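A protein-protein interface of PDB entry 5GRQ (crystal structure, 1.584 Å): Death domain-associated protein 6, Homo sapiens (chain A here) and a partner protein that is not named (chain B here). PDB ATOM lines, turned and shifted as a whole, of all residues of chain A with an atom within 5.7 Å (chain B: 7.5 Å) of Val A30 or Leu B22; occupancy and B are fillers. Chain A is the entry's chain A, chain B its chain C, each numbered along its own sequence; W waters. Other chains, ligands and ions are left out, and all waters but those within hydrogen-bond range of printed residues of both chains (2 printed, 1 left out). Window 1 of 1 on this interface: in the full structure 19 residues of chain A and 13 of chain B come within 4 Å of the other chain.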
ATOM      1  N   CYS A  20      16.850 -19.998 -24.011  1.00  0.00           N
ATOM      2  CA  CYS A  20      16.678 -19.930 -22.559  1.00  0.00           C
ATOM      3  C   CYS A  20      15.633 -18.889 -22.164  1.00  0.00           C
ATOM      4  O   CYS A  20      14.854 -19.116 -21.230  1.00  0.00           O
ATOM      5  CB  CYS A  20      18.016 -19.632 -21.890  1.00  0.00           C
ATOM      6  SG  CYS A  20      19.173 -21.005 -22.008  1.00  0.00           S
ATOM      7  N   THR A  24      12.793 -20.159 -19.597  1.00  0.00           N
ATOM      8  CA  THR A  24      13.173 -19.944 -18.202  1.00  0.00           C
ATOM      9  C   THR A  24      12.623 -18.631 -17.652  1.00  0.00           C
ATOM     10  O   THR A  24      13.249 -18.011 -16.783  1.00  0.00           O
ATOM     11  CB  THR A  24      14.698 -20.010 -18.020  1.00  0.00           C
ATOM     12  OG1 THR A  24      15.334 -18.948 -18.757  1.00  0.00           O
ATOM     13  CG2 THR A  24      15.234 -21.351 -18.478  1.00  0.00           C
ATOM     14  N   HIS A  27      12.635 -18.135 -13.952  1.00  0.00           N
ATOM     15  CA  HIS A  27      13.909 -17.907 -13.270  1.00  0.00           C
ATOM     16  C   HIS A  27      14.717 -16.940 -14.107  1.00  0.00           C
ATOM     17  O   HIS A  27      15.679 -17.320 -14.790  1.00  0.00           O
ATOM     18  CB  HIS A  27      14.632 -19.230 -12.991  1.00  0.00           C
ATOM     19  CG  HIS A  27      13.872 -20.076 -12.029  1.00  0.00           C
ATOM     20  ND1 HIS A  27      13.870 -19.832 -10.671  1.00  0.00           N
ATOM     21  CD2 HIS A  27      13.013 -21.102 -12.233  1.00  0.00           C
ATOM     22  CE1 HIS A  27      13.050 -20.685 -10.079  1.00  0.00           C
ATOM     23  NE2 HIS A  27      12.514 -21.461 -11.004  1.00  0.00           N
ATOM     24  N   PRO A  28      14.328 -15.659 -14.088  1.00  0.00           N
ATOM     25  CA  PRO A  28      14.985 -14.649 -14.934  1.00  0.00           C
ATOM     26  C   PRO A  28      16.463 -14.497 -14.670  1.00  0.00           C
ATOM     27  O   PRO A  28      17.133 -13.855 -15.478  1.00  0.00           O
ATOM     28  CB  PRO A  28      14.244 -13.346 -14.586  1.00  0.00           C
ATOM     29  CG  PRO A  28      13.061 -13.730 -13.770  1.00  0.00           C
ATOM     30  CD  PRO A  28      13.257 -15.106 -13.237  1.00  0.00           C
ATOM     31  N   GLU A  29      16.975 -15.045 -13.574  1.00  0.00           N
ATOM     32  CA  GLU A  29      18.387 -14.934 -13.247  1.00  0.00           C
ATOM     33  C   GLU A  29      19.264 -15.848 -14.096  1.00  0.00           C
ATOM     34  O   GLU A  29      20.483 -15.645 -14.140  1.00  0.00           O
ATOM     35  CB  GLU A  29      18.595 -15.234 -11.755  1.00  0.00           C
ATOM     36  CG  GLU A  29      18.430 -16.687 -11.349  1.00  0.00           C
ATOM     37  CD  GLU A  29      16.989 -17.095 -10.977  1.00  0.00           C
ATOM     38  OE1 GLU A  29      16.002 -16.440 -11.399  1.00  0.00           O
ATOM     39  OE2 GLU A  29      16.844 -18.092 -10.242  1.00  0.00           O
ATOM     40  N   VAL A  30      18.680 -16.838 -14.773  1.00  0.00           N
ATOM     41  CA  VAL A  30      19.488 -17.800 -15.529  1.00  0.00           C
ATOM     42  C   VAL A  30      20.204 -17.120 -16.689  1.00  0.00           C
ATOM     43  O   VAL A  30      21.424 -17.264 -16.869  1.00  0.00           O
ATOM     44  CB  VAL A  30      18.603 -18.963 -16.010  1.00  0.00           C
ATOM     45  CG1 VAL A  30      19.342 -19.817 -17.029  1.00  0.00           C
ATOM     46  CG2 VAL A  30      18.139 -19.804 -14.830  1.00  0.00           C
ATOM     47  N   VAL A  31      19.461 -16.376 -17.507  1.00  0.00           N
ATOM     48  CA  VAL A  31      20.057 -15.766 -18.694  1.00  0.00           C
ATOM     49  C   VAL A  31      21.174 -14.777 -18.348  1.00  0.00           C
ATOM     50  O   VAL A  31      22.274 -14.909 -18.903  1.00  0.00           O
ATOM     51  CB  VAL A  31      18.952 -15.166 -19.583  1.00  0.00           C
ATOM     52  CG1 VAL A  31      19.524 -14.156 -20.566  1.00  0.00           C
ATOM     53  CG2 VAL A  31      18.216 -16.300 -20.297  1.00  0.00           C
ATOM     54  N   PRO A  32      20.983 -13.813 -17.438  1.00  0.00           N
ATOM     55  CA  PRO A  32      22.115 -12.929 -17.098  1.00  0.00           C
ATOM     56  C   PRO A  32      23.298 -13.674 -16.505  1.00  0.00           C
ATOM     57  O   PRO A  32      24.449 -13.246 -16.676  1.00  0.00           O
ATOM     58  CB  PRO A  32      21.512 -11.949 -16.082  1.00  0.00           C
ATOM     59  CG  PRO A  32      20.050 -12.023 -16.267  1.00  0.00           C
ATOM     60  CD  PRO A  32      19.724 -13.367 -16.820  1.00  0.00           C
ATOM     61  N   PHE A  33      23.041 -14.772 -15.800  1.00  0.00           N
ATOM     62  CA  PHE A  33      24.125 -15.577 -15.249  1.00  0.00           C
ATOM     63  C   PHE A  33      24.981 -16.187 -16.358  1.00  0.00           C
ATOM     64  O   PHE A  33      26.216 -16.136 -16.294  1.00  0.00           O
ATOM     65  CB  PHE A  33      23.533 -16.660 -14.348  1.00  0.00           C
ATOM     66  CG  PHE A  33      24.533 -17.643 -13.868  1.00  0.00           C
ATOM     67  CD1 PHE A  33      25.290 -17.373 -12.738  1.00  0.00           C
ATOM     68  CD2 PHE A  33      24.715 -18.849 -14.528  1.00  0.00           C
ATOM     69  CE1 PHE A  33      26.217 -18.293 -12.281  1.00  0.00           C
ATOM     70  CE2 PHE A  33      25.645 -19.763 -14.073  1.00  0.00           C
ATOM     71  CZ  PHE A  33      26.385 -19.484 -12.946  1.00  0.00           C
ATOM     72  N   LEU A  34      24.344 -16.739 -17.395  1.00  0.00           N
ATOM     73  CA  LEU A  34      25.093 -17.308 -18.516  1.00  0.00           C
ATOM     74  C   LEU A  34      25.824 -16.227 -19.305  1.00  0.00           C
ATOM     75  O   LEU A  34      26.978 -16.413 -19.720  1.00  0.00           O
ATOM     76  CB  LEU A  34      24.135 -18.056 -19.442  1.00  0.00           C
ATOM     77  CG  LEU A  34      23.498 -19.301 -18.854  1.00  0.00           C
ATOM     78  CD1 LEU A  34      22.493 -19.867 -19.845  1.00  0.00           C
ATOM     79  CD2 LEU A  34      24.591 -20.323 -18.530  1.00  0.00           C
ATOM     80  N   TYR A  35      25.164 -15.088 -19.521  1.00  0.00           N
ATOM     81  CA  TYR A  35      25.816 -13.961 -20.170  1.00  0.00           C
ATOM     82  C   TYR A  35      27.061 -13.536 -19.401  1.00  0.00           C
ATOM     83  O   TYR A  35      28.109 -13.274 -20.001  1.00  0.00           O
ATOM     84  CB  TYR A  35      24.825 -12.799 -20.298  1.00  0.00           C
ATOM     85  CG  TYR A  35      25.438 -11.543 -20.844  1.00  0.00           C
ATOM     86  CD1 TYR A  35      25.637 -11.382 -22.214  1.00  0.00           C
ATOM     87  CD2 TYR A  35      25.815 -10.513 -19.995  1.00  0.00           C
ATOM     88  CE1 TYR A  35      26.202 -10.227 -22.717  1.00  0.00           C
ATOM     89  CE2 TYR A  35      26.387  -9.358 -20.496  1.00  0.00           C
ATOM     90  CZ  TYR A  35      26.576  -9.224 -21.853  1.00  0.00           C
ATOM     91  OH  TYR A  35      27.141  -8.071 -22.345  1.00  0.00           O
ATOM     92  N   TYR A  70      17.737 -27.904 -18.758  1.00  0.00           N
ATOM     93  CA  TYR A  70      18.660 -27.535 -17.690  1.00  0.00           C
ATOM     94  C   TYR A  70      19.880 -28.451 -17.644  1.00  0.00           C
ATOM     95  O   TYR A  70      20.953 -28.018 -17.208  1.00  0.00           O
ATOM     96  CB  TYR A  70      17.935 -27.519 -16.347  1.00  0.00           C
ATOM     97  CG  TYR A  70      17.188 -26.229 -16.078  1.00  0.00           C
ATOM     98  CD1 TYR A  70      17.836 -25.128 -15.530  1.00  0.00           C
ATOM     99  CD2 TYR A  70      15.835 -26.117 -16.366  1.00  0.00           C
ATOM    100  CE1 TYR A  70      17.155 -23.948 -15.270  1.00  0.00           C
ATOM    101  CE2 TYR A  70      15.151 -24.939 -16.112  1.00  0.00           C
ATOM    102  CZ  TYR A  70      15.817 -23.866 -15.561  1.00  0.00           C
ATOM    103  OH  TYR A  70      15.128 -22.699 -15.302  1.00  0.00           O
ATOM    104  N   ILE A  73      22.011 -26.609 -20.101  1.00  0.00           N
ATOM    105  CA  ILE A  73      22.491 -25.349 -19.534  1.00  0.00           C
ATOM    106  C   ILE A  73      23.660 -25.603 -18.591  1.00  0.00           C
ATOM    107  O   ILE A  73      24.668 -24.889 -18.624  1.00  0.00           O
ATOM    108  CB  ILE A  73      21.359 -24.586 -18.816  1.00  0.00           C
ATOM    109  CG1 ILE A  73      20.288 -24.145 -19.816  1.00  0.00           C
ATOM    110  CG2 ILE A  73      21.951 -23.362 -18.099  1.00  0.00           C
ATOM    111  CD1 ILE A  73      19.067 -23.453 -19.158  1.00  0.00           C
ATOM    112  N   ASP B   8       9.075 -28.269 -15.451  1.00  0.00           N
ATOM    113  CA  ASP B   8      10.425 -28.781 -15.641  1.00  0.00           C
ATOM    114  C   ASP B   8      10.644 -30.177 -15.060  1.00  0.00           C
ATOM    115  O   ASP B   8      11.755 -30.702 -15.167  1.00  0.00           O
ATOM    116  CB  ASP B   8      11.435 -27.810 -15.016  1.00  0.00           C
ATOM    117  CG  ASP B   8      11.387 -26.433 -15.648  1.00  0.00           C
ATOM    118  OD1 ASP B   8      11.414 -26.348 -16.899  1.00  0.00           O
ATOM    119  OD2 ASP B   8      11.305 -25.444 -14.889  1.00  0.00           O
ATOM    120  N   ILE B  16      17.002 -32.499 -11.340  1.00  0.00           N
ATOM    121  CA  ILE B  16      18.235 -32.420 -10.562  1.00  0.00           C
ATOM    122  C   ILE B  16      19.146 -31.325 -11.108  1.00  0.00           C
ATOM    123  O   ILE B  16      19.707 -30.525 -10.349  1.00  0.00           O
ATOM    124  CB  ILE B  16      18.933 -33.791 -10.556  1.00  0.00           C
ATOM    125  CG1 ILE B  16      18.068 -34.804  -9.809  1.00  0.00           C
ATOM    126  CG2 ILE B  16      20.329 -33.686  -9.966  1.00  0.00           C
ATOM    127  CD1 ILE B  16      18.501 -36.248 -10.016  1.00  0.00           C
ATOM    128  N   ALA B  17      19.315 -31.280 -12.430  1.00  0.00           N
ATOM    129  CA  ALA B  17      20.186 -30.274 -13.030  1.00  0.00           C
ATOM    130  C   ALA B  17      19.694 -28.869 -12.720  1.00  0.00           C
ATOM    131  O   ALA B  17      20.492 -27.967 -12.427  1.00  0.00           O
ATOM    132  CB  ALA B  17      20.264 -30.488 -14.543  1.00  0.00           C
ATOM    133  N   LYS B  18      18.379 -28.669 -12.778  1.00  0.00           N
ATOM    134  CA  LYS B  18      17.798 -27.366 -12.484  1.00  0.00           C
ATOM    135  C   LYS B  18      18.062 -26.957 -11.042  1.00  0.00           C
ATOM    136  O   LYS B  18      18.475 -25.824 -10.776  1.00  0.00           O
ATOM    137  CB  LYS B  18      16.291 -27.400 -12.766  1.00  0.00           C
ATOM    138  CG  LYS B  18      15.571 -26.108 -12.431  1.00  0.00           C
ATOM    139  CD  LYS B  18      14.079 -26.243 -12.727  1.00  0.00           C
ATOM    140  CE  LYS B  18      13.289 -25.066 -12.201  1.00  0.00           C
ATOM    141  NZ  LYS B  18      11.800 -25.336 -12.220  1.00  0.00           N
ATOM    142  N   LYS B  19      17.784 -27.856 -10.094  1.00  0.00           N
ATOM    143  CA  LYS B  19      18.017 -27.559  -8.682  1.00  0.00           C
ATOM    144  C   LYS B  19      19.466 -27.151  -8.447  1.00  0.00           C
ATOM    145  O   LYS B  19      19.747 -26.171  -7.746  1.00  0.00           O
ATOM    146  CB  LYS B  19      17.651 -28.775  -7.824  1.00  0.00           C
ATOM    147  CG  LYS B  19      17.728 -28.524  -6.326  1.00  0.00           C
ATOM    148  CD  LYS B  19      17.382 -29.791  -5.558  1.00  0.00           C
ATOM    149  CE  LYS B  19      16.365 -29.531  -4.454  1.00  0.00           C
ATOM    150  NZ  LYS B  19      16.933 -28.723  -3.340  1.00  0.00           N
ATOM    151  N   MET B  20      20.396 -27.879  -9.056  1.00  0.00           N
ATOM    152  CA  MET B  20      21.817 -27.599  -8.882  1.00  0.00           C
ATOM    153  C   MET B  20      22.185 -26.240  -9.464  1.00  0.00           C
ATOM    154  O   MET B  20      22.894 -25.447  -8.831  1.00  0.00           O
ATOM    155  CB  MET B  20      22.628 -28.715  -9.542  1.00  0.00           C
ATOM    156  CG  MET B  20      24.103 -28.722  -9.245  1.00  0.00           C
ATOM    157  SD  MET B  20      24.909 -30.031 -10.198  1.00  0.00           S
ATOM    158  CE  MET B  20      23.905 -31.453  -9.760  1.00  0.00           C
ATOM    159  N   LEU B  21      21.704 -25.950 -10.673  1.00  0.00           N
ATOM    160  CA  LEU B  21      22.042 -24.683 -11.309  1.00  0.00           C
ATOM    161  C   LEU B  21      21.487 -23.503 -10.525  1.00  0.00           C
ATOM    162  O   LEU B  21      22.200 -22.530 -10.272  1.00  0.00           O
ATOM    163  CB  LEU B  21      21.518 -24.663 -12.740  1.00  0.00           C
ATOM    164  CG  LEU B  21      21.843 -23.330 -13.415  1.00  0.00           C
ATOM    165  CD1 LEU B  21      23.353 -23.207 -13.706  1.00  0.00           C
ATOM    166  CD2 LEU B  21      21.017 -23.199 -14.679  1.00  0.00           C
ATOM    167  N   LEU B  22      20.208 -23.561 -10.138  1.00  0.00           N
ATOM    168  CA  LEU B  22      19.619 -22.435  -9.410  1.00  0.00           C
ATOM    169  C   LEU B  22      20.307 -22.200  -8.070  1.00  0.00           C
ATOM    170  O   LEU B  22      20.461 -21.049  -7.642  1.00  0.00           O
ATOM    171  CB  LEU B  22      18.117 -22.656  -9.210  1.00  0.00           C
ATOM    172  CG  LEU B  22      17.340 -22.716 -10.529  1.00  0.00           C
ATOM    173  CD1 LEU B  22      15.878 -22.902 -10.232  1.00  0.00           C
ATOM    174  CD2 LEU B  22      17.553 -21.459 -11.376  1.00  0.00           C
ATOM    175  N   GLU B  23      20.731 -23.269  -7.395  1.00  0.00           N
ATOM    176  CA  GLU B  23      21.483 -23.104  -6.154  1.00  0.00           C
ATOM    177  C   GLU B  23      22.833 -22.449  -6.418  1.00  0.00           C
ATOM    178  O   GLU B  23      23.275 -21.589  -5.643  1.00  0.00           O
ATOM    179  CB  GLU B  23      21.670 -24.456  -5.466  1.00  0.00           C
ATOM    180  CG  GLU B  23      20.427 -24.960  -4.747  1.00  0.00           C
ATOM    181  CD  GLU B  23      20.588 -26.376  -4.211  1.00  0.00           C
ATOM    182  OE1 GLU B  23      21.684 -26.957  -4.371  1.00  0.00           O
ATOM    183  OE2 GLU B  23      19.617 -26.909  -3.634  1.00  0.00           O
ATOM    184  N   GLU B  24      23.502 -22.852  -7.503  1.00  0.00           N
ATOM    185  CA  GLU B  24      24.763 -22.220  -7.875  1.00  0.00           C
ATOM    186  C   GLU B  24      24.574 -20.731  -8.115  1.00  0.00           C
ATOM    187  O   GLU B  24      25.365 -19.910  -7.634  1.00  0.00           O
ATOM    188  CB  GLU B  24      25.350 -22.879  -9.129  1.00  0.00           C
ATOM    189  CG  GLU B  24      26.595 -22.144  -9.663  1.00  0.00           C
ATOM    190  CD  GLU B  24      27.170 -22.748 -10.941  1.00  0.00           C
ATOM    191  OE1 GLU B  24      26.675 -23.794 -11.406  1.00  0.00           O
ATOM    192  OE2 GLU B  24      28.123 -22.157 -11.487  1.00  0.00           O
ATOM    193  N   ILE B  25      23.527 -20.364  -8.858  1.00  0.00           N
ATOM    194  CA  ILE B  25      23.328 -18.960  -9.213  1.00  0.00           C
ATOM    195  C   ILE B  25      23.031 -18.124  -7.972  1.00  0.00           C
ATOM    196  O   ILE B  25      23.562 -17.017  -7.808  1.00  0.00           O
ATOM    197  CB  ILE B  25      22.207 -18.830 -10.263  1.00  0.00           C
ATOM    198  CG1 ILE B  25      22.592 -19.542 -11.559  1.00  0.00           C
ATOM    199  CG2 ILE B  25      21.951 -17.362 -10.569  1.00  0.00           C
ATOM    200  CD1 ILE B  25      21.515 -19.502 -12.614  1.00  0.00           C
ATOM    201  N   LYS B  26      22.151 -18.630  -7.102  1.00  0.00           N
ATOM    202  CA  LYS B  26      21.767 -17.933  -5.876  1.00  0.00           C
ATOM    203  C   LYS B  26      22.980 -17.596  -5.015  1.00  0.00           C
ATOM    204  O   LYS B  26      23.018 -16.547  -4.357  1.00  0.00           O
ATOM    205  CB  LYS B  26      20.774 -18.819  -5.112  1.00  0.00           C
ATOM    206  CG  LYS B  26      20.402 -18.383  -3.718  1.00  0.00           C
ATOM    207  CD  LYS B  26      19.382 -19.356  -3.136  1.00  0.00           C
ATOM    208  CE  LYS B  26      18.999 -18.981  -1.723  1.00  0.00           C
ATOM    209  NZ  LYS B  26      18.152 -20.032  -1.099  1.00  0.00           N
ATOM    210  N   ALA B  27      23.985 -18.476  -5.013  1.00  0.00           N
ATOM    211  CA  ALA B  27      25.161 -18.296  -4.175  1.00  0.00           C
ATOM    212  C   ALA B  27      26.028 -17.119  -4.607  1.00  0.00           C
ATOM    213  O   ALA B  27      26.834 -16.636  -3.803  1.00  0.00           O
ATOM    214  CB  ALA B  27      25.989 -19.583  -4.165  1.00  0.00           C
ATOM    215  N   ASN B  28      25.882 -16.649  -5.845  1.00  0.00           N
ATOM    216  CA  ASN B  28      26.587 -15.461  -6.337  1.00  0.00           C
ATOM    217  C   ASN B  28      28.102 -15.621  -6.210  1.00  0.00           C
ATOM    218  O   ASN B  28      28.803 -14.752  -5.682  1.00  0.00           O
ATOM    219  CB  ASN B  28      26.108 -14.198  -5.611  1.00  0.00           C
ATOM    220  CG  ASN B  28      26.542 -12.922  -6.310  1.00  0.00           C
ATOM    221  OD1 ASN B  28      26.482 -12.833  -7.537  1.00  0.00           O
ATOM    222  ND2 ASN B  28      26.985 -11.929  -5.530  1.00  0.00           N
HETATM  223  O   HOH W   1      10.401 -23.219 -10.935  1.00  0.00           O
HETATM  224  O   HOH W   2      12.470 -22.932 -15.356  1.00  0.00           O
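Water W2 bridges OH of Tyr A70 (2.7 Å) and OD2 of Asp B8 (2.8 Å). Water W1 lies within hydrogen-bond range of a ring nitrogen (NE2) of His A27 (2.7 Å) and the side-chain amino group (NZ) of Lys B18 (2.8 Å).
Hydrophobic or aromatic side chains of chain A that line the printed part of chain B: His A27, Val A30, Phe A33, Tyr A70 and Ile A73.
The side-chain carboxylate (OD2) of Asp B8 is in salt-bridge range of the side-chain amino group (NZ) of Lys B18 (2.7 Å).
Printed residues of chain B within 4 Å of His A27: Lys B18 (3.9 Å) and Leu B22 (3.6 Å). Pro A28 touches none of the printed residues of chain B. Of the printed residues of chain B, Glu A29 touches Leu B22 and Ile B25. Val A30 touches just these residues of chain B: Leu B22 (3.9 Å) and Ile B25 (3.9 Å). Printed residues of chain B within 4 Å of Phe A33: Glu B24 (3.5 Å) and Ile B25 (3.6 Å). Printed residues of chain A within 4 Å of Lys B18: His A27 (3.9 Å) and Tyr A70 (3.6 Å). Of chain A, only His A27 (3.6 Å), Glu A29 (3.6 Å) and Val A30 (3.9 Å) come within 4 Å of Leu B22. Printed residues of chain A within 4 Å of Ile B25: Glu A29 (3.7 Å), Val A30 (3.9 Å) and Phe A33 (3.6 Å).
His A27 touches Lys B18. Leu B22 touches His A27. Glu A29 touches Leu B22. CG2 of Ile B25 touches CG of Glu A29, 3.7 Å away. CG2 of Val A30 touches CD2 of Leu B22, at 3.9 Å. Val A30 touches Ile B25 (CA to CD1, 3.9 Å). Phe A33 touches Glu B24 (CZ to OE2, 3.5 Å). Ala B17 touches Tyr A70 (CB to O, 3.7 Å). Tyr A70 touches Lys B18 (CG to CB, 3.6 Å). Ile A73 touches Leu B21 (CG2 to CD2, 3.5 Å).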
